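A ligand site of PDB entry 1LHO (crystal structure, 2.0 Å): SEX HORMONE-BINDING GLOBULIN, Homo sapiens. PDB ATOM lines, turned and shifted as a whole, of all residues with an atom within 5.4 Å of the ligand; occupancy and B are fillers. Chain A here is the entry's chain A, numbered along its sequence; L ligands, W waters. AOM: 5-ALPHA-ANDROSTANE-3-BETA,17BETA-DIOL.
Water W1 lies within hydrogen-bond range of O17 of the ligand (2.6 Å), NZ of Lys 134 (2.7 Å) and OG of Ser 128 (2.8 Å).
The backbone NH of Phe 67 lies within hydrogen-bond range of the backbone carbonyl oxygen of Gly 58.
The side-chain amino group (NZ) of Lys 134 lies within salt-bridge range of the side-chain carboxylate (OD2) of Asp 65.
The backbone carbonyl oxygen of Asp 65 is in hydrogen-bond range of the backbone NH of Thr 60 (3.1 Å).
OD1 of Asn 82 sits at hydrogen-bond distance from N of Trp 84, at 2.8 Å.
O of His 81 sits close to N of Asp 65 (3.4 Å).
OG1 of Thr 40 is in hydrogen-bond range of N of Met 107.
The side-chain hydroxyl (OG) of Ser 42 is in hydrogen-bond range of the backbone NH (N) of Leu 171 (3.1 Å).
The backbone carbonyl oxygen of His 81 lies within hydrogen-bond range of the backbone NH of Trp 66 (2.9 Å).
C of Ser 41 touches O3 of the ligand, at 3.6 Å.
Gly 58 touches the ligand.
CA of Asp 59 touches C15 of the ligand, at 3.97 Å.
N of Trp 66 touches C16 of the ligand (3.6 Å).
Phe 67 touches the ligand.
Met 107 touches the ligand (CG to C1, 3.7 Å).
Leu 131 touches the ligand (CD2 to C12, 3.9 Å).
NZ of Lys 134 touches O17 of the ligand, at 3.8 Å.
SD of Met 139 touches C7 of the ligand, 3.98 Å away.
Ile 141 touches the ligand (CD1 to C6, 3.9 Å).
CD2 of Leu 171 touches C3 of the ligand, 3.8 Å away.
Hydrophobic or aromatic side chains within 4 Å of the ligand: Phe 67, Met 107, Leu 131, Met 139, Ile 141 and Leu 171.
16 residues have an atom within 4 Å of the ligand: Thr 40, Ser 41, Ser 42, Gly 58, Asp 59, Asp 65, Trp 66, Phe 67, Asn 82, Val 105, Met 107, Leu 131, Lys 134, Met 139, Ile 141 and Leu 171.
The nearest printed residue that does not touch the ligand is Leu 80 (4.01 Å).
The backbone NH of Ser 42 sits close to an oxygen (O3) of the ligand (3.3 Å).
An oxygen (O17) of the ligand is in hydrogen-bond range of the side-chain carboxylate (OD1) of Asp 65, 2.7 Å away.
The backbone carbonyl oxygen (O) of Val 105 lies within hydrogen-bond range of an oxygen (O3) of the ligand.
OG of Ser 42 sits at hydrogen-bond distance from O3 of the ligand.
The backbone carbonyl oxygen (O) of Thr 40 sits at hydrogen-bond distance from an oxygen (O3) of the ligand (2.7 Å).
An oxygen (O17) of the ligand is in hydrogen-bond range of the side-chain amide nitrogen of Asn 82 (3.0 Å).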
ATOM      1  N   THR A  40     -22.899  10.070   5.470  1.00  0.00           N
ATOM      2  CA  THR A  40     -22.184  10.755   4.403  1.00  0.00           C
ATOM      3  C   THR A  40     -20.670  10.705   4.559  1.00  0.00           C
ATOM      4  O   THR A  40     -19.936  10.941   3.609  1.00  0.00           O
ATOM      5  CB  THR A  40     -22.533  12.247   4.329  1.00  0.00           C
ATOM      6  OG1 THR A  40     -21.927  12.920   5.446  1.00  0.00           O
ATOM      7  CG2 THR A  40     -24.044  12.449   4.346  1.00  0.00           C
ATOM      8  N   SER A  41     -20.200  10.381   5.755  1.00  0.00           N
ATOM      9  CA  SER A  41     -18.763  10.366   5.967  1.00  0.00           C
ATOM     10  C   SER A  41     -17.987   9.316   5.175  1.00  0.00           C
ATOM     11  O   SER A  41     -18.516   8.264   4.796  1.00  0.00           O
ATOM     12  CB  SER A  41     -18.464  10.194   7.456  1.00  0.00           C
ATOM     13  OG  SER A  41     -18.641   8.848   7.868  1.00  0.00           O
ATOM     14  N   SER A  42     -16.734   9.642   4.917  1.00  0.00           N
ATOM     15  CA  SER A  42     -15.808   8.760   4.239  1.00  0.00           C
ATOM     16  C   SER A  42     -14.520   8.908   5.043  1.00  0.00           C
ATOM     17  O   SER A  42     -14.170  10.016   5.474  1.00  0.00           O
ATOM     18  CB  SER A  42     -15.571   9.180   2.790  1.00  0.00           C
ATOM     19  OG  SER A  42     -16.744   9.065   2.019  1.00  0.00           O
ATOM     20  N   PHE A  56      -9.102  11.335  -3.827  1.00  0.00           N
ATOM     21  CA  PHE A  56     -10.392  10.859  -4.320  1.00  0.00           C
ATOM     22  C   PHE A  56     -11.218  12.001  -4.904  1.00  0.00           C
ATOM     23  O   PHE A  56     -11.014  13.185  -4.590  1.00  0.00           O
ATOM     24  CB  PHE A  56     -11.162  10.057  -3.238  1.00  0.00           C
ATOM     25  CG  PHE A  56     -11.964  10.894  -2.295  1.00  0.00           C
ATOM     26  CD1 PHE A  56     -13.239  11.329  -2.624  1.00  0.00           C
ATOM     27  CD2 PHE A  56     -11.461  11.202  -1.039  1.00  0.00           C
ATOM     28  CE1 PHE A  56     -14.020  12.055  -1.727  1.00  0.00           C
ATOM     29  CE2 PHE A  56     -12.218  11.929  -0.120  1.00  0.00           C
ATOM     30  CZ  PHE A  56     -13.505  12.356  -0.457  1.00  0.00           C
ATOM     31  N   GLY A  58     -15.367  13.028  -6.395  1.00  0.00           N
ATOM     32  CA  GLY A  58     -16.762  12.668  -6.287  1.00  0.00           C
ATOM     33  C   GLY A  58     -17.635  13.620  -7.071  1.00  0.00           C
ATOM     34  O   GLY A  58     -17.301  14.798  -7.208  1.00  0.00           O
ATOM     35  N   ASP A  59     -18.758  13.124  -7.602  1.00  0.00           N
ATOM     36  CA  ASP A  59     -19.698  13.964  -8.343  1.00  0.00           C
ATOM     37  C   ASP A  59     -21.074  13.320  -8.498  1.00  0.00           C
ATOM     38  O   ASP A  59     -21.280  12.181  -8.095  1.00  0.00           O
ATOM     39  CB  ASP A  59     -19.148  14.315  -9.755  1.00  0.00           C
ATOM     40  CG  ASP A  59     -19.223  13.139 -10.779  1.00  0.00           C
ATOM     41  OD1 ASP A  59     -20.000  12.184 -10.601  1.00  0.00           O
ATOM     42  OD2 ASP A  59     -18.491  13.213 -11.797  1.00  0.00           O
ATOM     43  N   THR A  60     -22.017  14.103  -9.027  1.00  0.00           N
ATOM     44  CA  THR A  60     -23.345  13.620  -9.392  1.00  0.00           C
ATOM     45  C   THR A  60     -23.436  14.113 -10.835  1.00  0.00           C
ATOM     46  O   THR A  60     -24.371  13.759 -11.550  1.00  0.00           O
ATOM     47  CB  THR A  60     -24.516  14.278  -8.623  1.00  0.00           C
ATOM     48  OG1 THR A  60     -24.606  15.668  -8.969  1.00  0.00           O
ATOM     49  CG2 THR A  60     -24.361  14.091  -7.132  1.00  0.00           C
ATOM     50  N   ASP A  65     -21.229  19.603 -10.736  1.00  0.00           N
ATOM     51  CA  ASP A  65     -21.530  19.137  -9.398  1.00  0.00           C
ATOM     52  C   ASP A  65     -20.467  18.117  -9.065  1.00  0.00           C
ATOM     53  O   ASP A  65     -20.738  16.916  -9.062  1.00  0.00           O
ATOM     54  CB  ASP A  65     -22.920  18.511  -9.291  1.00  0.00           C
ATOM     55  CG  ASP A  65     -23.363  18.365  -7.851  1.00  0.00           C
ATOM     56  OD1 ASP A  65     -23.143  19.320  -7.077  1.00  0.00           O
ATOM     57  OD2 ASP A  65     -23.912  17.309  -7.480  1.00  0.00           O
ATOM     58  N   TRP A  66     -19.262  18.600  -8.806  1.00  0.00           N
ATOM     59  CA  TRP A  66     -18.137  17.725  -8.493  1.00  0.00           C
ATOM     60  C   TRP A  66     -17.282  18.193  -7.313  1.00  0.00           C
ATOM     61  O   TRP A  66     -17.404  19.316  -6.826  1.00  0.00           O
ATOM     62  CB  TRP A  66     -17.281  17.509  -9.754  1.00  0.00           C
ATOM     63  CG  TRP A  66     -16.633  18.760 -10.302  1.00  0.00           C
ATOM     64  CD1 TRP A  66     -17.118  19.562 -11.308  1.00  0.00           C
ATOM     65  CD2 TRP A  66     -15.376  19.318  -9.923  1.00  0.00           C
ATOM     66  NE1 TRP A  66     -16.220  20.581 -11.570  1.00  0.00           N
ATOM     67  CE2 TRP A  66     -15.158  20.460 -10.729  1.00  0.00           C
ATOM     68  CE3 TRP A  66     -14.413  18.967  -8.961  1.00  0.00           C
ATOM     69  CZ2 TRP A  66     -14.005  21.245 -10.608  1.00  0.00           C
ATOM     70  CZ3 TRP A  66     -13.261  19.752  -8.841  1.00  0.00           C
ATOM     71  CH2 TRP A  66     -13.073  20.880  -9.670  1.00  0.00           C
ATOM     72  N   PHE A  67     -16.398  17.295  -6.864  1.00  0.00           N
ATOM     73  CA  PHE A  67     -15.535  17.538  -5.708  1.00  0.00           C
ATOM     74  C   PHE A  67     -14.245  16.760  -5.864  1.00  0.00           C
ATOM     75  O   PHE A  67     -14.233  15.668  -6.426  1.00  0.00           O
ATOM     76  CB  PHE A  67     -16.265  17.052  -4.453  1.00  0.00           C
ATOM     77  CG  PHE A  67     -15.407  16.986  -3.199  1.00  0.00           C
ATOM     78  CD1 PHE A  67     -15.504  17.975  -2.210  1.00  0.00           C
ATOM     79  CD2 PHE A  67     -14.591  15.869  -2.947  1.00  0.00           C
ATOM     80  CE1 PHE A  67     -14.811  17.853  -0.987  1.00  0.00           C
ATOM     81  CE2 PHE A  67     -13.887  15.734  -1.739  1.00  0.00           C
ATOM     82  CZ  PHE A  67     -14.005  16.734  -0.755  1.00  0.00           C
ATOM     83  N   LEU A  80     -13.937  22.229  -5.366  1.00  0.00           N
ATOM     84  CA  LEU A  80     -15.344  21.866  -5.348  1.00  0.00           C
ATOM     85  C   LEU A  80     -16.064  22.799  -6.284  1.00  0.00           C
ATOM     86  O   LEU A  80     -15.745  23.988  -6.348  1.00  0.00           O
ATOM     87  CB  LEU A  80     -15.846  22.012  -3.889  1.00  0.00           C
ATOM     88  CG  LEU A  80     -17.277  21.938  -3.363  1.00  0.00           C
ATOM     89  CD1 LEU A  80     -17.230  21.646  -1.850  1.00  0.00           C
ATOM     90  CD2 LEU A  80     -18.016  23.234  -3.645  1.00  0.00           C
ATOM     91  N   HIS A  81     -17.028  22.256  -7.031  1.00  0.00           N
ATOM     92  CA  HIS A  81     -17.810  23.061  -7.953  1.00  0.00           C
ATOM     93  C   HIS A  81     -19.244  22.597  -7.992  1.00  0.00           C
ATOM     94  O   HIS A  81     -19.539  21.479  -8.448  1.00  0.00           O
ATOM     95  CB  HIS A  81     -17.211  23.014  -9.372  1.00  0.00           C
ATOM     96  CG  HIS A  81     -17.928  23.893 -10.354  1.00  0.00           C
ATOM     97  ND1 HIS A  81     -17.426  25.105 -10.771  1.00  0.00           N
ATOM     98  CD2 HIS A  81     -19.111  23.732 -10.984  1.00  0.00           C
ATOM     99  CE1 HIS A  81     -18.285  25.671 -11.610  1.00  0.00           C
ATOM    100  NE2 HIS A  81     -19.316  24.849 -11.754  1.00  0.00           N
ATOM    101  N   ASN A  82     -20.148  23.435  -7.498  1.00  0.00           N
ATOM    102  CA  ASN A  82     -21.575  23.120  -7.538  1.00  0.00           C
ATOM    103  C   ASN A  82     -22.406  24.397  -7.595  1.00  0.00           C
ATOM    104  O   ASN A  82     -21.863  25.507  -7.721  1.00  0.00           O
ATOM    105  CB  ASN A  82     -22.009  22.240  -6.343  1.00  0.00           C
ATOM    106  CG  ASN A  82     -21.809  22.902  -4.986  1.00  0.00           C
ATOM    107  OD1 ASN A  82     -21.899  24.124  -4.841  1.00  0.00           O
ATOM    108  ND2 ASN A  82     -21.577  22.078  -3.975  1.00  0.00           N
ATOM    109  N   TRP A  84     -23.912  26.032  -5.389  1.00  0.00           N
ATOM    110  CA  TRP A  84     -23.674  26.968  -4.289  1.00  0.00           C
ATOM    111  C   TRP A  84     -22.275  27.551  -4.129  1.00  0.00           C
ATOM    112  O   TRP A  84     -22.099  28.645  -3.614  1.00  0.00           O
ATOM    113  CB  TRP A  84     -24.043  26.290  -2.961  1.00  0.00           C
ATOM    114  CG  TRP A  84     -25.436  25.769  -2.938  1.00  0.00           C
ATOM    115  CD1 TRP A  84     -26.578  26.489  -2.711  1.00  0.00           C
ATOM    116  CD2 TRP A  84     -25.858  24.418  -3.168  1.00  0.00           C
ATOM    117  NE1 TRP A  84     -27.677  25.671  -2.768  1.00  0.00           N
ATOM    118  CE2 TRP A  84     -27.263  24.389  -3.049  1.00  0.00           C
ATOM    119  CE3 TRP A  84     -25.171  23.229  -3.463  1.00  0.00           C
ATOM    120  CZ2 TRP A  84     -27.999  23.211  -3.219  1.00  0.00           C
ATOM    121  CZ3 TRP A  84     -25.903  22.055  -3.620  1.00  0.00           C
ATOM    122  CH2 TRP A  84     -27.309  22.051  -3.502  1.00  0.00           C
ATOM    123  N   VAL A 105     -13.665  12.810   5.761  1.00  0.00           N
ATOM    124  CA  VAL A 105     -14.412  13.855   5.088  1.00  0.00           C
ATOM    125  C   VAL A 105     -15.882  13.610   5.333  1.00  0.00           C
ATOM    126  O   VAL A 105     -16.374  12.494   5.115  1.00  0.00           O
ATOM    127  CB  VAL A 105     -14.191  13.868   3.555  1.00  0.00           C
ATOM    128  CG1 VAL A 105     -15.009  15.001   2.932  1.00  0.00           C
ATOM    129  CG2 VAL A 105     -12.700  14.030   3.222  1.00  0.00           C
ATOM    130  N   LYS A 106     -16.599  14.626   5.790  1.00  0.00           N
ATOM    131  CA  LYS A 106     -18.010  14.456   6.009  1.00  0.00           C
ATOM    132  C   LYS A 106     -18.818  15.733   5.903  1.00  0.00           C
ATOM    133  O   LYS A 106     -18.265  16.838   5.880  1.00  0.00           O
ATOM    134  CB  LYS A 106     -18.258  13.809   7.378  1.00  0.00           C
ATOM    135  CG  LYS A 106     -17.829  14.656   8.552  1.00  0.00           C
ATOM    136  CD  LYS A 106     -18.014  13.870   9.852  1.00  0.00           C
ATOM    137  CE  LYS A 106     -17.589  14.685  11.055  1.00  0.00           C
ATOM    138  NZ  LYS A 106     -17.699  13.873  12.306  1.00  0.00           N
ATOM    139  N   MET A 107     -20.121  15.548   5.826  1.00  0.00           N
ATOM    140  CA  MET A 107     -21.069  16.640   5.743  1.00  0.00           C
ATOM    141  C   MET A 107     -21.522  16.979   7.162  1.00  0.00           C
ATOM    142  O   MET A 107     -21.718  16.088   7.980  1.00  0.00           O
ATOM    143  CB  MET A 107     -22.295  16.220   4.944  1.00  0.00           C
ATOM    144  CG  MET A 107     -22.042  16.051   3.473  1.00  0.00           C
ATOM    145  SD  MET A 107     -21.659  17.648   2.791  1.00  0.00           S
ATOM    146  CE  MET A 107     -23.333  18.316   2.611  1.00  0.00           C
ATOM    147  N   VAL A 112     -18.773  21.006   4.508  1.00  0.00           N
ATOM    148  CA  VAL A 112     -17.935  19.848   4.242  1.00  0.00           C
ATOM    149  C   VAL A 112     -16.758  20.000   5.212  1.00  0.00           C
ATOM    150  O   VAL A 112     -16.051  21.018   5.196  1.00  0.00           O
ATOM    151  CB  VAL A 112     -17.422  19.817   2.777  1.00  0.00           C
ATOM    152  CG1 VAL A 112     -16.369  18.723   2.615  1.00  0.00           C
ATOM    153  CG2 VAL A 112     -18.587  19.538   1.816  1.00  0.00           C
ATOM    154  N   VAL A 127     -21.652  25.198   1.480  1.00  0.00           N
ATOM    155  CA  VAL A 127     -21.347  24.656   0.166  1.00  0.00           C
ATOM    156  C   VAL A 127     -22.310  23.599  -0.355  1.00  0.00           C
ATOM    157  O   VAL A 127     -22.207  23.195  -1.510  1.00  0.00           O
ATOM    158  CB  VAL A 127     -19.888  24.112   0.085  1.00  0.00           C
ATOM    159  CG1 VAL A 127     -18.909  25.222   0.437  1.00  0.00           C
ATOM    160  CG2 VAL A 127     -19.708  22.939   1.003  1.00  0.00           C
ATOM    161  N   SER A 128     -23.269  23.171   0.462  1.00  0.00           N
ATOM    162  CA  SER A 128     -24.185  22.150  -0.009  1.00  0.00           C
ATOM    163  C   SER A 128     -25.461  21.943   0.795  1.00  0.00           C
ATOM    164  O   SER A 128     -25.493  22.155   2.003  1.00  0.00           O
ATOM    165  CB  SER A 128     -23.469  20.808  -0.085  1.00  0.00           C
ATOM    166  OG  SER A 128     -24.379  19.797  -0.514  1.00  0.00           O
ATOM    167  N   LEU A 131     -27.674  15.837   0.946  1.00  0.00           N
ATOM    168  CA  LEU A 131     -27.366  14.960  -0.192  1.00  0.00           C
ATOM    169  C   LEU A 131     -28.591  14.196  -0.691  1.00  0.00           C
ATOM    170  O   LEU A 131     -28.906  14.224  -1.875  1.00  0.00           O
ATOM    171  CB  LEU A 131     -26.282  13.942   0.181  1.00  0.00           C
ATOM    172  CG  LEU A 131     -24.868  14.456   0.503  1.00  0.00           C
ATOM    173  CD1 LEU A 131     -23.964  13.260   0.767  1.00  0.00           C
ATOM    174  CD2 LEU A 131     -24.345  15.287  -0.651  1.00  0.00           C
ATOM    175  N   LYS A 134     -30.845  15.858  -3.234  1.00  0.00           N
ATOM    176  CA  LYS A 134     -30.232  16.439  -4.425  1.00  0.00           C
ATOM    177  C   LYS A 134     -30.947  16.027  -5.708  1.00  0.00           C
ATOM    178  O   LYS A 134     -31.612  14.986  -5.754  1.00  0.00           O
ATOM    179  CB  LYS A 134     -28.749  16.018  -4.503  1.00  0.00           C
ATOM    180  CG  LYS A 134     -27.854  16.668  -3.459  1.00  0.00           C
ATOM    181  CD  LYS A 134     -26.417  16.116  -3.497  1.00  0.00           C
ATOM    182  CE  LYS A 134     -25.746  16.314  -4.865  1.00  0.00           C
ATOM    183  NZ  LYS A 134     -25.603  17.745  -5.231  1.00  0.00           N
ATOM    184  N   MET A 139     -24.466   9.327  -7.085  1.00  0.00           N
ATOM    185  CA  MET A 139     -23.148   9.886  -6.800  1.00  0.00           C
ATOM    186  C   MET A 139     -22.044   8.892  -7.136  1.00  0.00           C
ATOM    187  O   MET A 139     -22.115   7.704  -6.789  1.00  0.00           O
ATOM    188  CB  MET A 139     -23.016  10.246  -5.316  1.00  0.00           C
ATOM    189  CG  MET A 139     -21.659  10.865  -4.947  1.00  0.00           C
ATOM    190  SD  MET A 139     -21.632  11.508  -3.242  1.00  0.00           S
ATOM    191  CE  MET A 139     -22.650  12.901  -3.449  1.00  0.00           C
ATOM    192  N   ILE A 141     -17.918   7.979  -6.791  1.00  0.00           N
ATOM    193  CA  ILE A 141     -16.702   8.247  -6.021  1.00  0.00           C
ATOM    194  C   ILE A 141     -15.557   7.535  -6.753  1.00  0.00           C
ATOM    195  O   ILE A 141     -15.632   6.325  -6.977  1.00  0.00           O
ATOM    196  CB  ILE A 141     -16.729   7.672  -4.576  1.00  0.00           C
ATOM    197  CG1 ILE A 141     -17.834   8.306  -3.734  1.00  0.00           C
ATOM    198  CG2 ILE A 141     -15.371   7.931  -3.901  1.00  0.00           C
ATOM    199  CD1 ILE A 141     -17.690   9.800  -3.520  1.00  0.00           C
ATOM    200  N   LEU A 171     -18.828   6.767   2.074  1.00  0.00           N
ATOM    201  CA  LEU A 171     -20.237   7.119   2.238  1.00  0.00           C
ATOM    202  C   LEU A 171     -21.007   6.027   2.972  1.00  0.00           C
ATOM    203  O   LEU A 171     -20.601   5.579   4.046  1.00  0.00           O
ATOM    204  CB  LEU A 171     -20.875   7.392   0.876  1.00  0.00           C
ATOM    205  CG  LEU A 171     -20.493   8.710   0.193  1.00  0.00           C
ATOM    206  CD1 LEU A 171     -20.788   8.642  -1.298  1.00  0.00           C
ATOM    207  CD2 LEU A 171     -21.240   9.869   0.847  1.00  0.00           C
HETATM  208  C1  AOM L   1     -19.710  14.493   1.071  1.00  0.00           C
HETATM  209  C10 AOM L   1     -18.971  14.719  -0.284  1.00  0.00           C
HETATM  210  C11 AOM L   1     -20.473  16.798  -0.865  1.00  0.00           C
HETATM  211  C12 AOM L   1     -21.423  17.462  -1.929  1.00  0.00           C
HETATM  212  C13 AOM L   1     -20.741  17.591  -3.300  1.00  0.00           C
HETATM  213  C14 AOM L   1     -20.215  16.195  -3.764  1.00  0.00           C
HETATM  214  C15 AOM L   1     -19.778  16.435  -5.236  1.00  0.00           C
HETATM  215  C16 AOM L   1     -20.814  17.542  -5.730  1.00  0.00           C
HETATM  216  C17 AOM L   1     -21.676  17.835  -4.495  1.00  0.00           C
HETATM  217  C18 AOM L   1     -19.629  18.696  -3.233  1.00  0.00           C
HETATM  218  C19 AOM L   1     -17.742  15.674   0.002  1.00  0.00           C
HETATM  219  C2  AOM L   1     -18.837  13.711   2.111  1.00  0.00           C
HETATM  220  C3  AOM L   1     -18.397  12.357   1.489  1.00  0.00           C
HETATM  221  C4  AOM L   1     -17.604  12.561   0.162  1.00  0.00           C
HETATM  222  C5  AOM L   1     -18.487  13.306  -0.861  1.00  0.00           C
HETATM  223  C6  AOM L   1     -17.754  13.503  -2.211  1.00  0.00           C
HETATM  224  C7  AOM L   1     -18.686  14.185  -3.225  1.00  0.00           C
HETATM  225  C8  AOM L   1     -19.214  15.573  -2.749  1.00  0.00           C
HETATM  226  C9  AOM L   1     -19.923  15.415  -1.343  1.00  0.00           C
HETATM  227  O3  AOM L   1     -17.595  11.636   2.437  1.00  0.00           O
HETATM  228  O17 AOM L   1     -22.183  19.178  -4.568  1.00  0.00           O
HETATM  229  O   HOH W   1     -24.474  19.146  -3.250  1.00  0.00           O
